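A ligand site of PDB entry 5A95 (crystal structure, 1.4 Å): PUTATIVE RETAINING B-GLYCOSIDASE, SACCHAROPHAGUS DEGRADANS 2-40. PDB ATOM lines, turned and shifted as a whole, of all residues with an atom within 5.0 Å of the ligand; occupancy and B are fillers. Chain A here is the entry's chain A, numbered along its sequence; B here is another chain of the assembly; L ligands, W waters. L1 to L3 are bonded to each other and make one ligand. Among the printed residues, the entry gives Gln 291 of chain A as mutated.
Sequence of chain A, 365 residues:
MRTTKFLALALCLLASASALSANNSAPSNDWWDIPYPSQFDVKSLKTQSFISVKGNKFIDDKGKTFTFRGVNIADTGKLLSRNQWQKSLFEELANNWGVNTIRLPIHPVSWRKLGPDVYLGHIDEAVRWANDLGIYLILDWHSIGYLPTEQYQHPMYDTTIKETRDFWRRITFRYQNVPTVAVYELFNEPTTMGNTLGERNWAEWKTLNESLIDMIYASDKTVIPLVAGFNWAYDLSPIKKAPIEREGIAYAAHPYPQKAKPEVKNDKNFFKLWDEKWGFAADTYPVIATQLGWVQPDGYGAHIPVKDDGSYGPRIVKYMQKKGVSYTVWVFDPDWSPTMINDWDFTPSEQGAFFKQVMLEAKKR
O of Trp 32 of chain B sits at hydrogen-bond distance from O5 of LG3 L3 (3.3 Å). O of Ser 337 is in hydrogen-bond range of O1 of LG2 L2. An oxygen (O1) of LG3 L3 sits at hydrogen-bond distance from the backbone NH of Ser 337 (2.9 Å). OG of Ser 337 lies within hydrogen-bond range of O1 of LG3 L3. The side-chain amide nitrogen of Gln 291 sits at hydrogen-bond distance from an oxygen (O2) of LIG L1, 3.3 Å away. ND2 of Asn 188 lies within hydrogen-bond range of O2 of LIG L1, 3.3 Å away. O2 of LG3 L3 sits at hydrogen-bond distance from OH of Tyr 300 (3.2 Å). The side-chain carboxylate (OE1) of Glu 189 sits at hydrogen-bond distance from an oxygen (O1) of LIG L1, at 2.6 Å. O of Asp 335 lies within hydrogen-bond range of O1 of LG3 L3, at 2.7 Å. An oxygen (O3) of LIG L1 lies within hydrogen-bond range of a ring nitrogen (NE2) of His 142. A ring nitrogen (NE2) of His 107 sits at hydrogen-bond distance from an oxygen (O5) of LG2 L2, at 2.7 Å. The side-chain sulfur of Met 156 is in hydrogen-bond range of an oxygen (O5) of LG2 L2, at 3.7 Å. NE2 of His 303 sits at hydrogen-bond distance from O6 of LIG L1 (2.6 Å). The indole nitrogen (NE1) of Trp 330 lies within hydrogen-bond range of an oxygen (O4) of LIG L1 (3.2 Å). OH of Tyr 157 is in hydrogen-bond range of O5 of LG2 L2 (2.6 Å).
OG of Ser 337 sits at hydrogen-bond distance from O of Gly 301, 3.4 Å away. The side-chain amide oxygen (OE1) of Gln 291 sits close to the side-chain amide oxygen (OD1) of Asn 188, 3.1 Å away. A ring nitrogen (ND1) of His 303 is in hydrogen-bond range of the backbone carbonyl oxygen of Gly 301, at 2.6 Å. The side-chain hydroxyl of Tyr 300 lies within hydrogen-bond range of the backbone carbonyl oxygen of Asp 335 (2.7 Å). OH of Tyr 157 lies within hydrogen-bond range of SD of Met 156, 3.6 Å away. O of Ser 337 sits at hydrogen-bond distance from NE1 of Trp 330 (3.1 Å). The side-chain amide nitrogen of Asn 188 lies close to a ring nitrogen (NE2) of His 142, 3.4 Å away. The side-chain amide nitrogen of Gln 291 sits at hydrogen-bond distance from the side-chain hydroxyl of Tyr 256 (2.9 Å).
Merely in contact with the ligand: Val 306 (3.4 Å), Trp 336 (3.5 Å) and Ile 144 (3.6 Å). Hydrophobic or aromatic side chains that line the ligand: His 107, His 142, Ile 144, Met 156, Tyr 157, Tyr 300, His 303, Val 306, Trp 330, Trp 336 and Trp 32 of chain B. 16 residues have an atom within 4 Å of the ligand: His 107, His 142, Ile 144, Met 156, Tyr 157, Asn 188, Glu 189, Gln 291, Tyr 300, His 303, Val 306, Trp 330, Asp 335, Trp 336, Ser 337 and Trp 32 of chain B. The nearest printed residue that does not touch the ligand is Tyr 256 (4.1 Å).
Water W8 bridges the side-chain carboxylate (OD1) of Asp 33 of chain B (2.5 Å) and an oxygen (O5) of LG3 L3 (2.6 Å). Water W9 lies within hydrogen-bond range of an oxygen (O3) of LG2 L2 (2.7 Å) and the backbone carbonyl oxygen (O) of Trp 32 of chain B (2.9 Å). Water W4 lies within hydrogen-bond range of the backbone carbonyl oxygen of Trp 32 of chain B (3.0 Å) and an oxygen (O5) of LG3 L3 (3.2 Å). Water W11 bridges O5 of LIG L1 and NE2 of His 303. Water W6 lies within hydrogen-bond range of the side-chain carboxylate of Glu 189 (2.9 Å) and an oxygen (O1) of LIG L1 (3.2 Å).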
ATOM      1  N   HIS A 107      20.271 -25.360  14.465  1.00  0.00           N
ATOM      2  CA  HIS A 107      21.265 -24.502  15.074  1.00  0.00           C
ATOM      3  C   HIS A 107      20.764 -23.977  16.419  1.00  0.00           C
ATOM      4  O   HIS A 107      19.660 -23.459  16.494  1.00  0.00           O
ATOM      5  CB  HIS A 107      21.594 -23.317  14.173  1.00  0.00           C
ATOM      6  CG  HIS A 107      22.426 -23.689  12.993  1.00  0.00           C
ATOM      7  ND1 HIS A 107      22.101 -24.700  12.119  1.00  0.00           N
ATOM      8  CD2 HIS A 107      23.596 -23.169  12.536  1.00  0.00           C
ATOM      9  CE1 HIS A 107      23.015 -24.768  11.159  1.00  0.00           C
ATOM     10  NE2 HIS A 107      23.932 -23.849  11.400  1.00  0.00           N
ATOM     11  N   HIS A 142      23.028 -28.930  15.923  1.00  0.00           N
ATOM     12  CA  HIS A 142      24.092 -28.476  15.034  1.00  0.00           C
ATOM     13  C   HIS A 142      24.954 -27.398  15.704  1.00  0.00           C
ATOM     14  O   HIS A 142      24.832 -26.206  15.439  1.00  0.00           O
ATOM     15  CB  HIS A 142      23.519 -28.012  13.710  1.00  0.00           C
ATOM     16  CG  HIS A 142      24.525 -27.907  12.635  1.00  0.00           C
ATOM     17  ND1 HIS A 142      24.878 -28.971  11.847  1.00  0.00           N
ATOM     18  CD2 HIS A 142      25.292 -26.861  12.230  1.00  0.00           C
ATOM     19  CE1 HIS A 142      25.791 -28.582  10.980  1.00  0.00           C
ATOM     20  NE2 HIS A 142      26.061 -27.310  11.185  1.00  0.00           N
ATOM     21  N   ILE A 144      29.216 -26.645  16.941  1.00  0.00           N
ATOM     22  CA  ILE A 144      30.610 -26.862  16.555  1.00  0.00           C
ATOM     23  C   ILE A 144      31.438 -26.326  17.706  1.00  0.00           C
ATOM     24  O   ILE A 144      31.394 -25.115  17.987  1.00  0.00           O
ATOM     25  CB  ILE A 144      30.995 -26.112  15.258  1.00  0.00           C
ATOM     26  CG1 ILE A 144      30.064 -26.482  14.107  1.00  0.00           C
ATOM     27  CG2 ILE A 144      32.447 -26.433  14.920  1.00  0.00           C
ATOM     28  CD1 ILE A 144      30.420 -25.849  12.781  1.00  0.00           C
ATOM     29  N   MET A 156      26.624 -18.665  16.599  1.00  0.00           N
ATOM     30  CA  MET A 156      25.442 -19.335  16.081  1.00  0.00           C
ATOM     31  C   MET A 156      25.307 -20.776  16.632  1.00  0.00           C
ATOM     32  O   MET A 156      24.203 -21.350  16.646  1.00  0.00           O
ATOM     33  CB  MET A 156      25.384 -19.331  14.555  1.00  0.00           C
ATOM     34  CG  MET A 156      26.463 -20.173  13.865  1.00  0.00           C
ATOM     35  SD  MET A 156      26.251 -20.176  12.058  1.00  0.00           S
ATOM     36  CE  MET A 156      26.906 -18.577  11.653  1.00  0.00           C
ATOM     37  N   TYR A 157      26.432 -21.327  17.084  1.00  0.00           N
ATOM     38  CA  TYR A 157      26.513 -22.644  17.621  1.00  0.00           C
ATOM     39  C   TYR A 157      26.461 -22.698  19.141  1.00  0.00           C
ATOM     40  O   TYR A 157      26.500 -23.770  19.748  1.00  0.00           O
ATOM     41  CB  TYR A 157      27.818 -23.289  17.157  1.00  0.00           C
ATOM     42  CG  TYR A 157      27.984 -23.254  15.658  1.00  0.00           C
ATOM     43  CD1 TYR A 157      27.016 -23.774  14.805  1.00  0.00           C
ATOM     44  CD2 TYR A 157      29.099 -22.683  15.092  1.00  0.00           C
ATOM     45  CE1 TYR A 157      27.170 -23.683  13.415  1.00  0.00           C
ATOM     46  CE2 TYR A 157      29.283 -22.607  13.720  1.00  0.00           C
ATOM     47  CZ  TYR A 157      28.306 -23.101  12.877  1.00  0.00           C
ATOM     48  OH  TYR A 157      28.448 -23.006  11.506  1.00  0.00           O
ATOM     49  N   ASN A 188      26.760 -32.137  16.467  1.00  0.00           N
ATOM     50  CA  ASN A 188      27.307 -32.145  15.105  1.00  0.00           C
ATOM     51  C   ASN A 188      28.826 -32.332  15.019  1.00  0.00           C
ATOM     52  O   ASN A 188      29.332 -33.321  14.484  1.00  0.00           O
ATOM     53  CB  ASN A 188      26.842 -30.860  14.436  1.00  0.00           C
ATOM     54  CG  ASN A 188      27.531 -30.550  13.132  1.00  0.00           C
ATOM     55  OD1 ASN A 188      27.575 -31.328  12.199  1.00  0.00           O
ATOM     56  ND2 ASN A 188      28.059 -29.325  13.055  1.00  0.00           N
ATOM     57  N   GLU A 189      29.593 -31.345  15.484  1.00  0.00           N
ATOM     58  CA  GLU A 189      31.040 -31.330  15.257  1.00  0.00           C
ATOM     59  C   GLU A 189      31.833 -30.991  16.510  1.00  0.00           C
ATOM     60  O   GLU A 189      32.132 -29.800  16.783  1.00  0.00           O
ATOM     61  CB  GLU A 189      31.421 -30.398  14.097  1.00  0.00           C
ATOM     62  CG  GLU A 189      31.180 -31.075  12.747  1.00  0.00           C
ATOM     63  CD  GLU A 189      31.549 -30.246  11.556  1.00  0.00           C
ATOM     64  OE1 GLU A 189      31.634 -29.020  11.689  1.00  0.00           O
ATOM     65  OE2 GLU A 189      31.701 -30.847  10.469  1.00  0.00           O
ATOM     66  N   TRP A 232      36.342 -32.059  14.310  1.00  0.00           N
ATOM     67  CA  TRP A 232      35.110 -31.778  13.591  1.00  0.00           C
ATOM     68  C   TRP A 232      34.450 -33.062  13.080  1.00  0.00           C
ATOM     69  O   TRP A 232      34.162 -33.212  11.884  1.00  0.00           O
ATOM     70  CB  TRP A 232      35.320 -30.782  12.450  1.00  0.00           C
ATOM     71  CG  TRP A 232      35.663 -29.365  12.849  1.00  0.00           C
ATOM     72  CD1 TRP A 232      34.789 -28.323  12.880  1.00  0.00           C
ATOM     73  CD2 TRP A 232      36.942 -28.840  13.194  1.00  0.00           C
ATOM     74  NE1 TRP A 232      35.436 -27.157  13.220  1.00  0.00           N
ATOM     75  CE2 TRP A 232      36.766 -27.436  13.405  1.00  0.00           C
ATOM     76  CE3 TRP A 232      38.215 -29.375  13.296  1.00  0.00           C
ATOM     77  CZ2 TRP A 232      37.802 -26.598  13.784  1.00  0.00           C
ATOM     78  CZ3 TRP A 232      39.256 -28.528  13.675  1.00  0.00           C
ATOM     79  CH2 TRP A 232      39.047 -27.165  13.903  1.00  0.00           C
ATOM     80  N   TYR A 256      35.177 -34.486   4.647  1.00  0.00           N
ATOM     81  CA  TYR A 256      35.404 -33.512   3.594  1.00  0.00           C
ATOM     82  C   TYR A 256      36.751 -33.782   2.888  1.00  0.00           C
ATOM     83  O   TYR A 256      37.641 -34.420   3.463  1.00  0.00           O
ATOM     84  CB  TYR A 256      35.313 -32.141   4.188  1.00  0.00           C
ATOM     85  CG  TYR A 256      33.901 -31.647   4.448  1.00  0.00           C
ATOM     86  CD1 TYR A 256      32.989 -31.517   3.415  1.00  0.00           C
ATOM     87  CD2 TYR A 256      33.506 -31.221   5.707  1.00  0.00           C
ATOM     88  CE1 TYR A 256      31.718 -31.018   3.620  1.00  0.00           C
ATOM     89  CE2 TYR A 256      32.252 -30.686   5.914  1.00  0.00           C
ATOM     90  CZ  TYR A 256      31.356 -30.595   4.874  1.00  0.00           C
ATOM     91  OH  TYR A 256      30.098 -30.059   5.117  1.00  0.00           O
ATOM     92  N   GLN A 291      28.012 -35.268   6.968  1.00  0.00           N
ATOM     93  CA  GLN A 291      28.436 -34.171   6.102  1.00  0.00           C
ATOM     94  C   GLN A 291      29.578 -34.673   5.276  1.00  0.00           C
ATOM     95  O   GLN A 291      30.492 -35.350   5.750  1.00  0.00           O
ATOM     96  CB  GLN A 291      28.870 -32.930   6.869  1.00  0.00           C
ATOM     97  CG  GLN A 291      27.714 -32.330   7.624  1.00  0.00           C
ATOM     98  CD  GLN A 291      27.988 -31.015   8.315  1.00  0.00           C
ATOM     99  OE1 GLN A 291      27.263 -30.646   9.217  1.00  0.00           O
ATOM    100  NE2 GLN A 291      28.935 -30.264   7.818  1.00  0.00           N
ATOM    101  N   TYR A 300      32.027 -21.042  -5.502  1.00  0.00           N
ATOM    102  CA  TYR A 300      31.150 -20.366  -4.575  1.00  0.00           C
ATOM    103  C   TYR A 300      31.381 -20.827  -3.122  1.00  0.00           C
ATOM    104  O   TYR A 300      31.308 -22.013  -2.774  1.00  0.00           O
ATOM    105  CB  TYR A 300      29.665 -20.534  -4.982  1.00  0.00           C
ATOM    106  CG  TYR A 300      28.732 -19.913  -3.986  1.00  0.00           C
ATOM    107  CD1 TYR A 300      28.493 -18.549  -3.982  1.00  0.00           C
ATOM    108  CD2 TYR A 300      28.079 -20.683  -3.031  1.00  0.00           C
ATOM    109  CE1 TYR A 300      27.641 -17.973  -3.024  1.00  0.00           C
ATOM    110  CE2 TYR A 300      27.247 -20.116  -2.074  1.00  0.00           C
ATOM    111  CZ  TYR A 300      27.033 -18.762  -2.084  1.00  0.00           C
ATOM    112  OH  TYR A 300      26.185 -18.197  -1.155  1.00  0.00           O
ATOM    113  N   GLY A 301      31.743 -19.874  -2.292  1.00  0.00           N
ATOM    114  CA  GLY A 301      31.986 -20.140  -0.897  1.00  0.00           C
ATOM    115  C   GLY A 301      33.140 -21.048  -0.561  1.00  0.00           C
ATOM    116  O   GLY A 301      33.205 -21.561   0.516  1.00  0.00           O
ATOM    117  N   HIS A 303      36.402 -22.852   0.685  1.00  0.00           N
ATOM    118  CA  HIS A 303      37.204 -22.733   1.879  1.00  0.00           C
ATOM    119  C   HIS A 303      37.736 -24.123   2.252  1.00  0.00           C
ATOM    120  O   HIS A 303      37.142 -25.114   1.897  1.00  0.00           O
ATOM    121  CB  HIS A 303      36.330 -22.232   3.044  1.00  0.00           C
ATOM    122  CG  HIS A 303      35.103 -23.068   3.288  1.00  0.00           C
ATOM    123  ND1 HIS A 303      33.932 -22.924   2.563  1.00  0.00           N
ATOM    124  CD2 HIS A 303      34.859 -24.049   4.189  1.00  0.00           C
ATOM    125  CE1 HIS A 303      33.022 -23.776   3.005  1.00  0.00           C
ATOM    126  NE2 HIS A 303      33.565 -24.476   4.002  1.00  0.00           N
ATOM    127  N   PRO A 305      37.899 -27.102   4.702  1.00  0.00           N
ATOM    128  CA  PRO A 305      38.462 -28.263   4.029  1.00  0.00           C
ATOM    129  C   PRO A 305      37.625 -28.817   2.877  1.00  0.00           C
ATOM    130  O   PRO A 305      37.670 -30.029   2.618  1.00  0.00           O
ATOM    131  CB  PRO A 305      38.501 -29.282   5.171  1.00  0.00           C
ATOM    132  CG  PRO A 305      37.208 -29.036   5.880  1.00  0.00           C
ATOM    133  CD  PRO A 305      37.045 -27.518   5.841  1.00  0.00           C
ATOM    134  N   VAL A 306      36.848 -27.984   2.185  1.00  0.00           N
ATOM    135  CA  VAL A 306      35.902 -28.452   1.187  1.00  0.00           C
ATOM    136  C   VAL A 306      36.325 -28.215  -0.270  1.00  0.00           C
ATOM    137  O   VAL A 306      35.554 -28.503  -1.181  1.00  0.00           O
ATOM    138  CB  VAL A 306      34.476 -27.863   1.398  1.00  0.00           C
ATOM    139  CG1 VAL A 306      34.013 -28.168   2.811  1.00  0.00           C
ATOM    140  CG2 VAL A 306      34.397 -26.362   1.133  1.00  0.00           C
ATOM    141  N   TRP A 330      26.315 -32.399   2.265  1.00  0.00           N
ATOM    142  CA  TRP A 330      26.170 -31.007   2.686  1.00  0.00           C
ATOM    143  C   TRP A 330      26.440 -30.111   1.468  1.00  0.00           C
ATOM    144  O   TRP A 330      27.526 -30.196   0.921  1.00  0.00           O
ATOM    145  CB  TRP A 330      27.179 -30.682   3.834  1.00  0.00           C
ATOM    146  CG  TRP A 330      27.083 -29.261   4.341  1.00  0.00           C
ATOM    147  CD1 TRP A 330      27.669 -28.161   3.796  1.00  0.00           C
ATOM    148  CD2 TRP A 330      26.282 -28.800   5.427  1.00  0.00           C
ATOM    149  NE1 TRP A 330      27.327 -27.045   4.502  1.00  0.00           N
ATOM    150  CE2 TRP A 330      26.464 -27.396   5.514  1.00  0.00           C
ATOM    151  CE3 TRP A 330      25.436 -29.429   6.349  1.00  0.00           C
ATOM    152  CZ2 TRP A 330      25.815 -26.614   6.461  1.00  0.00           C
ATOM    153  CZ3 TRP A 330      24.799 -28.662   7.287  1.00  0.00           C
ATOM    154  CH2 TRP A 330      25.002 -27.256   7.365  1.00  0.00           C
ATOM    155  N   ASP A 335      22.556 -21.051  -0.782  1.00  0.00           N
ATOM    156  CA  ASP A 335      23.284 -20.014  -0.059  1.00  0.00           C
ATOM    157  C   ASP A 335      24.413 -20.562   0.801  1.00  0.00           C
ATOM    158  O   ASP A 335      25.545 -20.064   0.742  1.00  0.00           O
ATOM    159  CB  ASP A 335      22.341 -19.187   0.835  1.00  0.00           C
ATOM    160  CG  ASP A 335      21.209 -18.598   0.068  1.00  0.00           C
ATOM    161  OD1 ASP A 335      21.487 -17.944  -0.943  1.00  0.00           O
ATOM    162  OD2 ASP A 335      20.037 -18.785   0.450  1.00  0.00           O
ATOM    163  N   TRP A 336      24.131 -21.587   1.583  1.00  0.00           N
ATOM    164  CA  TRP A 336      25.109 -22.221   2.435  1.00  0.00           C
ATOM    165  C   TRP A 336      25.972 -23.158   1.608  1.00  0.00           C
ATOM    166  O   TRP A 336      25.454 -23.888   0.773  1.00  0.00           O
ATOM    167  CB  TRP A 336      24.380 -23.006   3.524  1.00  0.00           C
ATOM    168  CG  TRP A 336      23.777 -22.172   4.576  1.00  0.00           C
ATOM    169  CD1 TRP A 336      23.648 -20.803   4.597  1.00  0.00           C
ATOM    170  CD2 TRP A 336      23.239 -22.644   5.813  1.00  0.00           C
ATOM    171  NE1 TRP A 336      23.069 -20.401   5.790  1.00  0.00           N
ATOM    172  CE2 TRP A 336      22.779 -21.520   6.541  1.00  0.00           C
ATOM    173  CE3 TRP A 336      23.074 -23.919   6.363  1.00  0.00           C
ATOM    174  CZ2 TRP A 336      22.207 -21.628   7.795  1.00  0.00           C
ATOM    175  CZ3 TRP A 336      22.507 -24.030   7.648  1.00  0.00           C
ATOM    176  CH2 TRP A 336      22.079 -22.897   8.341  1.00  0.00           C
ATOM    177  N   SER A 337      27.277 -23.155   1.865  1.00  0.00           N
ATOM    178  CA  SER A 337      28.227 -23.834   1.005  1.00  0.00           C
ATOM    179  C   SER A 337      28.966 -24.970   1.741  1.00  0.00           C
ATOM    180  O   SER A 337      29.051 -24.973   2.972  1.00  0.00           O
ATOM    181  CB  SER A 337      29.247 -22.828   0.470  1.00  0.00           C
ATOM    182  OG  SER A 337      29.993 -22.274   1.528  1.00  0.00           O
ATOM    183  N   PRO A 338      29.503 -25.952   1.001  1.00  0.00           N
ATOM    184  CA  PRO A 338      29.360 -26.111  -0.447  1.00  0.00           C
ATOM    185  C   PRO A 338      27.917 -26.451  -0.849  1.00  0.00           C
ATOM    186  O   PRO A 338      27.298 -27.319  -0.253  1.00  0.00           O
ATOM    187  CB  PRO A 338      30.310 -27.272  -0.771  1.00  0.00           C
ATOM    188  CG  PRO A 338      30.415 -28.052   0.504  1.00  0.00           C
ATOM    189  CD  PRO A 338      30.395 -26.984   1.566  1.00  0.00           C
ATOM    190  N   TRP B  32      23.128 -16.220  10.496  1.00  0.00           N
ATOM    191  CA  TRP B  32      24.109 -16.981   9.703  1.00  0.00           C
ATOM    192  C   TRP B  32      25.057 -16.034   8.960  1.00  0.00           C
ATOM    193  O   TRP B  32      26.046 -16.491   8.410  1.00  0.00           O
ATOM    194  CB  TRP B  32      23.452 -17.995   8.748  1.00  0.00           C
ATOM    195  CG  TRP B  32      22.477 -17.391   7.796  1.00  0.00           C
ATOM    196  CD1 TRP B  32      22.724 -16.911   6.540  1.00  0.00           C
ATOM    197  CD2 TRP B  32      21.094 -17.174   8.052  1.00  0.00           C
ATOM    198  NE1 TRP B  32      21.578 -16.413   6.006  1.00  0.00           N
ATOM    199  CE2 TRP B  32      20.542 -16.573   6.899  1.00  0.00           C
ATOM    200  CE3 TRP B  32      20.256 -17.463   9.147  1.00  0.00           C
ATOM    201  CZ2 TRP B  32      19.212 -16.200   6.817  1.00  0.00           C
ATOM    202  CZ3 TRP B  32      18.927 -17.102   9.073  1.00  0.00           C
ATOM    203  CH2 TRP B  32      18.415 -16.475   7.908  1.00  0.00           C
ATOM    204  N   ASP B  33      24.757 -14.719   8.958  1.00  0.00           N
ATOM    205  CA  ASP B  33      25.608 -13.712   8.344  1.00  0.00           C
ATOM    206  C   ASP B  33      26.532 -13.015   9.354  1.00  0.00           C
ATOM    207  O   ASP B  33      27.300 -12.157   8.980  1.00  0.00           O
ATOM    208  CB  ASP B  33      24.768 -12.631   7.642  1.00  0.00           C
ATOM    209  CG  ASP B  33      24.012 -13.153   6.437  1.00  0.00           C
ATOM    210  OD1 ASP B  33      24.528 -14.050   5.705  1.00  0.00           O
ATOM    211  OD2 ASP B  33      22.893 -12.616   6.218  1.00  0.00           O
HETATM  212  C1  LIG L   1      29.873 -27.048   9.412  1.00  0.00           C
HETATM  213  C2  LIG L   1      28.829 -26.415   8.489  1.00  0.00           C
HETATM  214  C3  LIG L   1      29.534 -25.544   7.445  1.00  0.00           C
HETATM  215  C4  LIG L   1      30.577 -26.357   6.712  1.00  0.00           C
HETATM  216  C5  LIG L   1      31.302 -25.559   5.650  1.00  0.00           C
HETATM  217  C6  LIG L   1      31.094 -27.612   8.680  1.00  0.00           C
HETATM  218  O1  LIG L   1      32.225 -27.732   9.510  1.00  0.00           O
HETATM  219  O2  LIG L   1      29.241 -28.064  10.261  1.00  0.00           O
HETATM  220  O3  LIG L   1      27.870 -25.710   9.337  1.00  0.00           O
HETATM  221  O4  LIG L   1      28.682 -24.917   6.475  1.00  0.00           O
HETATM  222  O5  LIG L   1      31.559 -26.735   7.683  1.00  0.00           O
HETATM  223  O6  LIG L   1      32.368 -26.395   5.207  1.00  0.00           O
HETATM  224  C1  LG2 L   2      28.116 -22.807   5.483  1.00  0.00           C
HETATM  225  C2  LG2 L   2      27.822 -21.370   5.871  1.00  0.00           C
HETATM  226  C3  LG2 L   2      26.709 -21.304   6.892  1.00  0.00           C
HETATM  227  C4  LG2 L   2      27.017 -22.214   8.082  1.00  0.00           C
HETATM  228  C5  LG2 L   2      25.855 -22.376   9.034  1.00  0.00           C
HETATM  229  C6  LG2 L   2      28.449 -23.557   6.769  1.00  0.00           C
HETATM  230  O1  LG2 L   2      29.226 -22.789   4.587  1.00  0.00           O
HETATM  231  O2  LG2 L   2      27.396 -20.671   4.695  1.00  0.00           O
HETATM  232  O3  LG2 L   2      26.609 -19.967   7.368  1.00  0.00           O
HETATM  233  O4  LG2 L   2      27.322 -23.522   7.619  1.00  0.00           O
HETATM  234  O5  LG2 L   2      26.228 -23.265  10.085  1.00  0.00           O
HETATM  235  C1  LG3 L   3      27.953 -19.239   2.841  1.00  0.00           C
HETATM  236  C2  LG3 L   3      28.870 -18.156   2.328  1.00  0.00           C
HETATM  237  C3  LG3 L   3      28.992 -17.051   3.356  1.00  0.00           C
HETATM  238  C4  LG3 L   3      29.460 -17.632   4.667  1.00  0.00           C
HETATM  239  C5  LG3 L   3      29.550 -16.560   5.769  1.00  0.00           C
HETATM  240  C6  LG3 L   3      28.367 -19.722   4.202  1.00  0.00           C
HETATM  241  O1  LG3 L   3      27.958 -20.329   1.916  1.00  0.00           O
HETATM  242  O2  LG3 L   3      28.322 -17.611   1.137  1.00  0.00           O
HETATM  243  O3  LG3 L   3      29.910 -16.067   2.852  1.00  0.00           O
HETATM  244  O4  LG3 L   3      28.509 -18.609   5.109  1.00  0.00           O
HETATM  245  O5  LG3 L   3      28.248 -16.016   6.013  1.00  0.00           O
HETATM  246  O   HOH W   1      33.144 -25.012  10.092  1.00  0.00           O
HETATM  247  O   HOH W   2      30.078 -16.757  -0.648  1.00  0.00           O
HETATM  248  O   HOH W   3      29.340 -13.541   3.420  1.00  0.00           O
HETATM  249  O   HOH W   4      28.921 -16.076   9.129  1.00  0.00           O
HETATM  250  O   HOH W   5      31.510 -21.347   5.073  1.00  0.00           O
HETATM  251  O   HOH W   6      34.155 -30.280   8.951  1.00  0.00           O
HETATM  252  O   HOH W   7      31.401 -15.218   7.956  1.00  0.00           O
HETATM  253  O   HOH W   8      26.897 -14.163   4.828  1.00  0.00           O
HETATM  254  O   HOH W   9      25.867 -17.857   5.880  1.00  0.00           O
HETATM  255  O   HOH W  10      34.168 -27.981   7.018  1.00  0.00           O
HETATM  256  O   HOH W  11      34.062 -24.734   7.423  1.00  0.00           O
HETATM  257  O   HOH W  12      28.913 -18.854   8.657  1.00  0.00           O
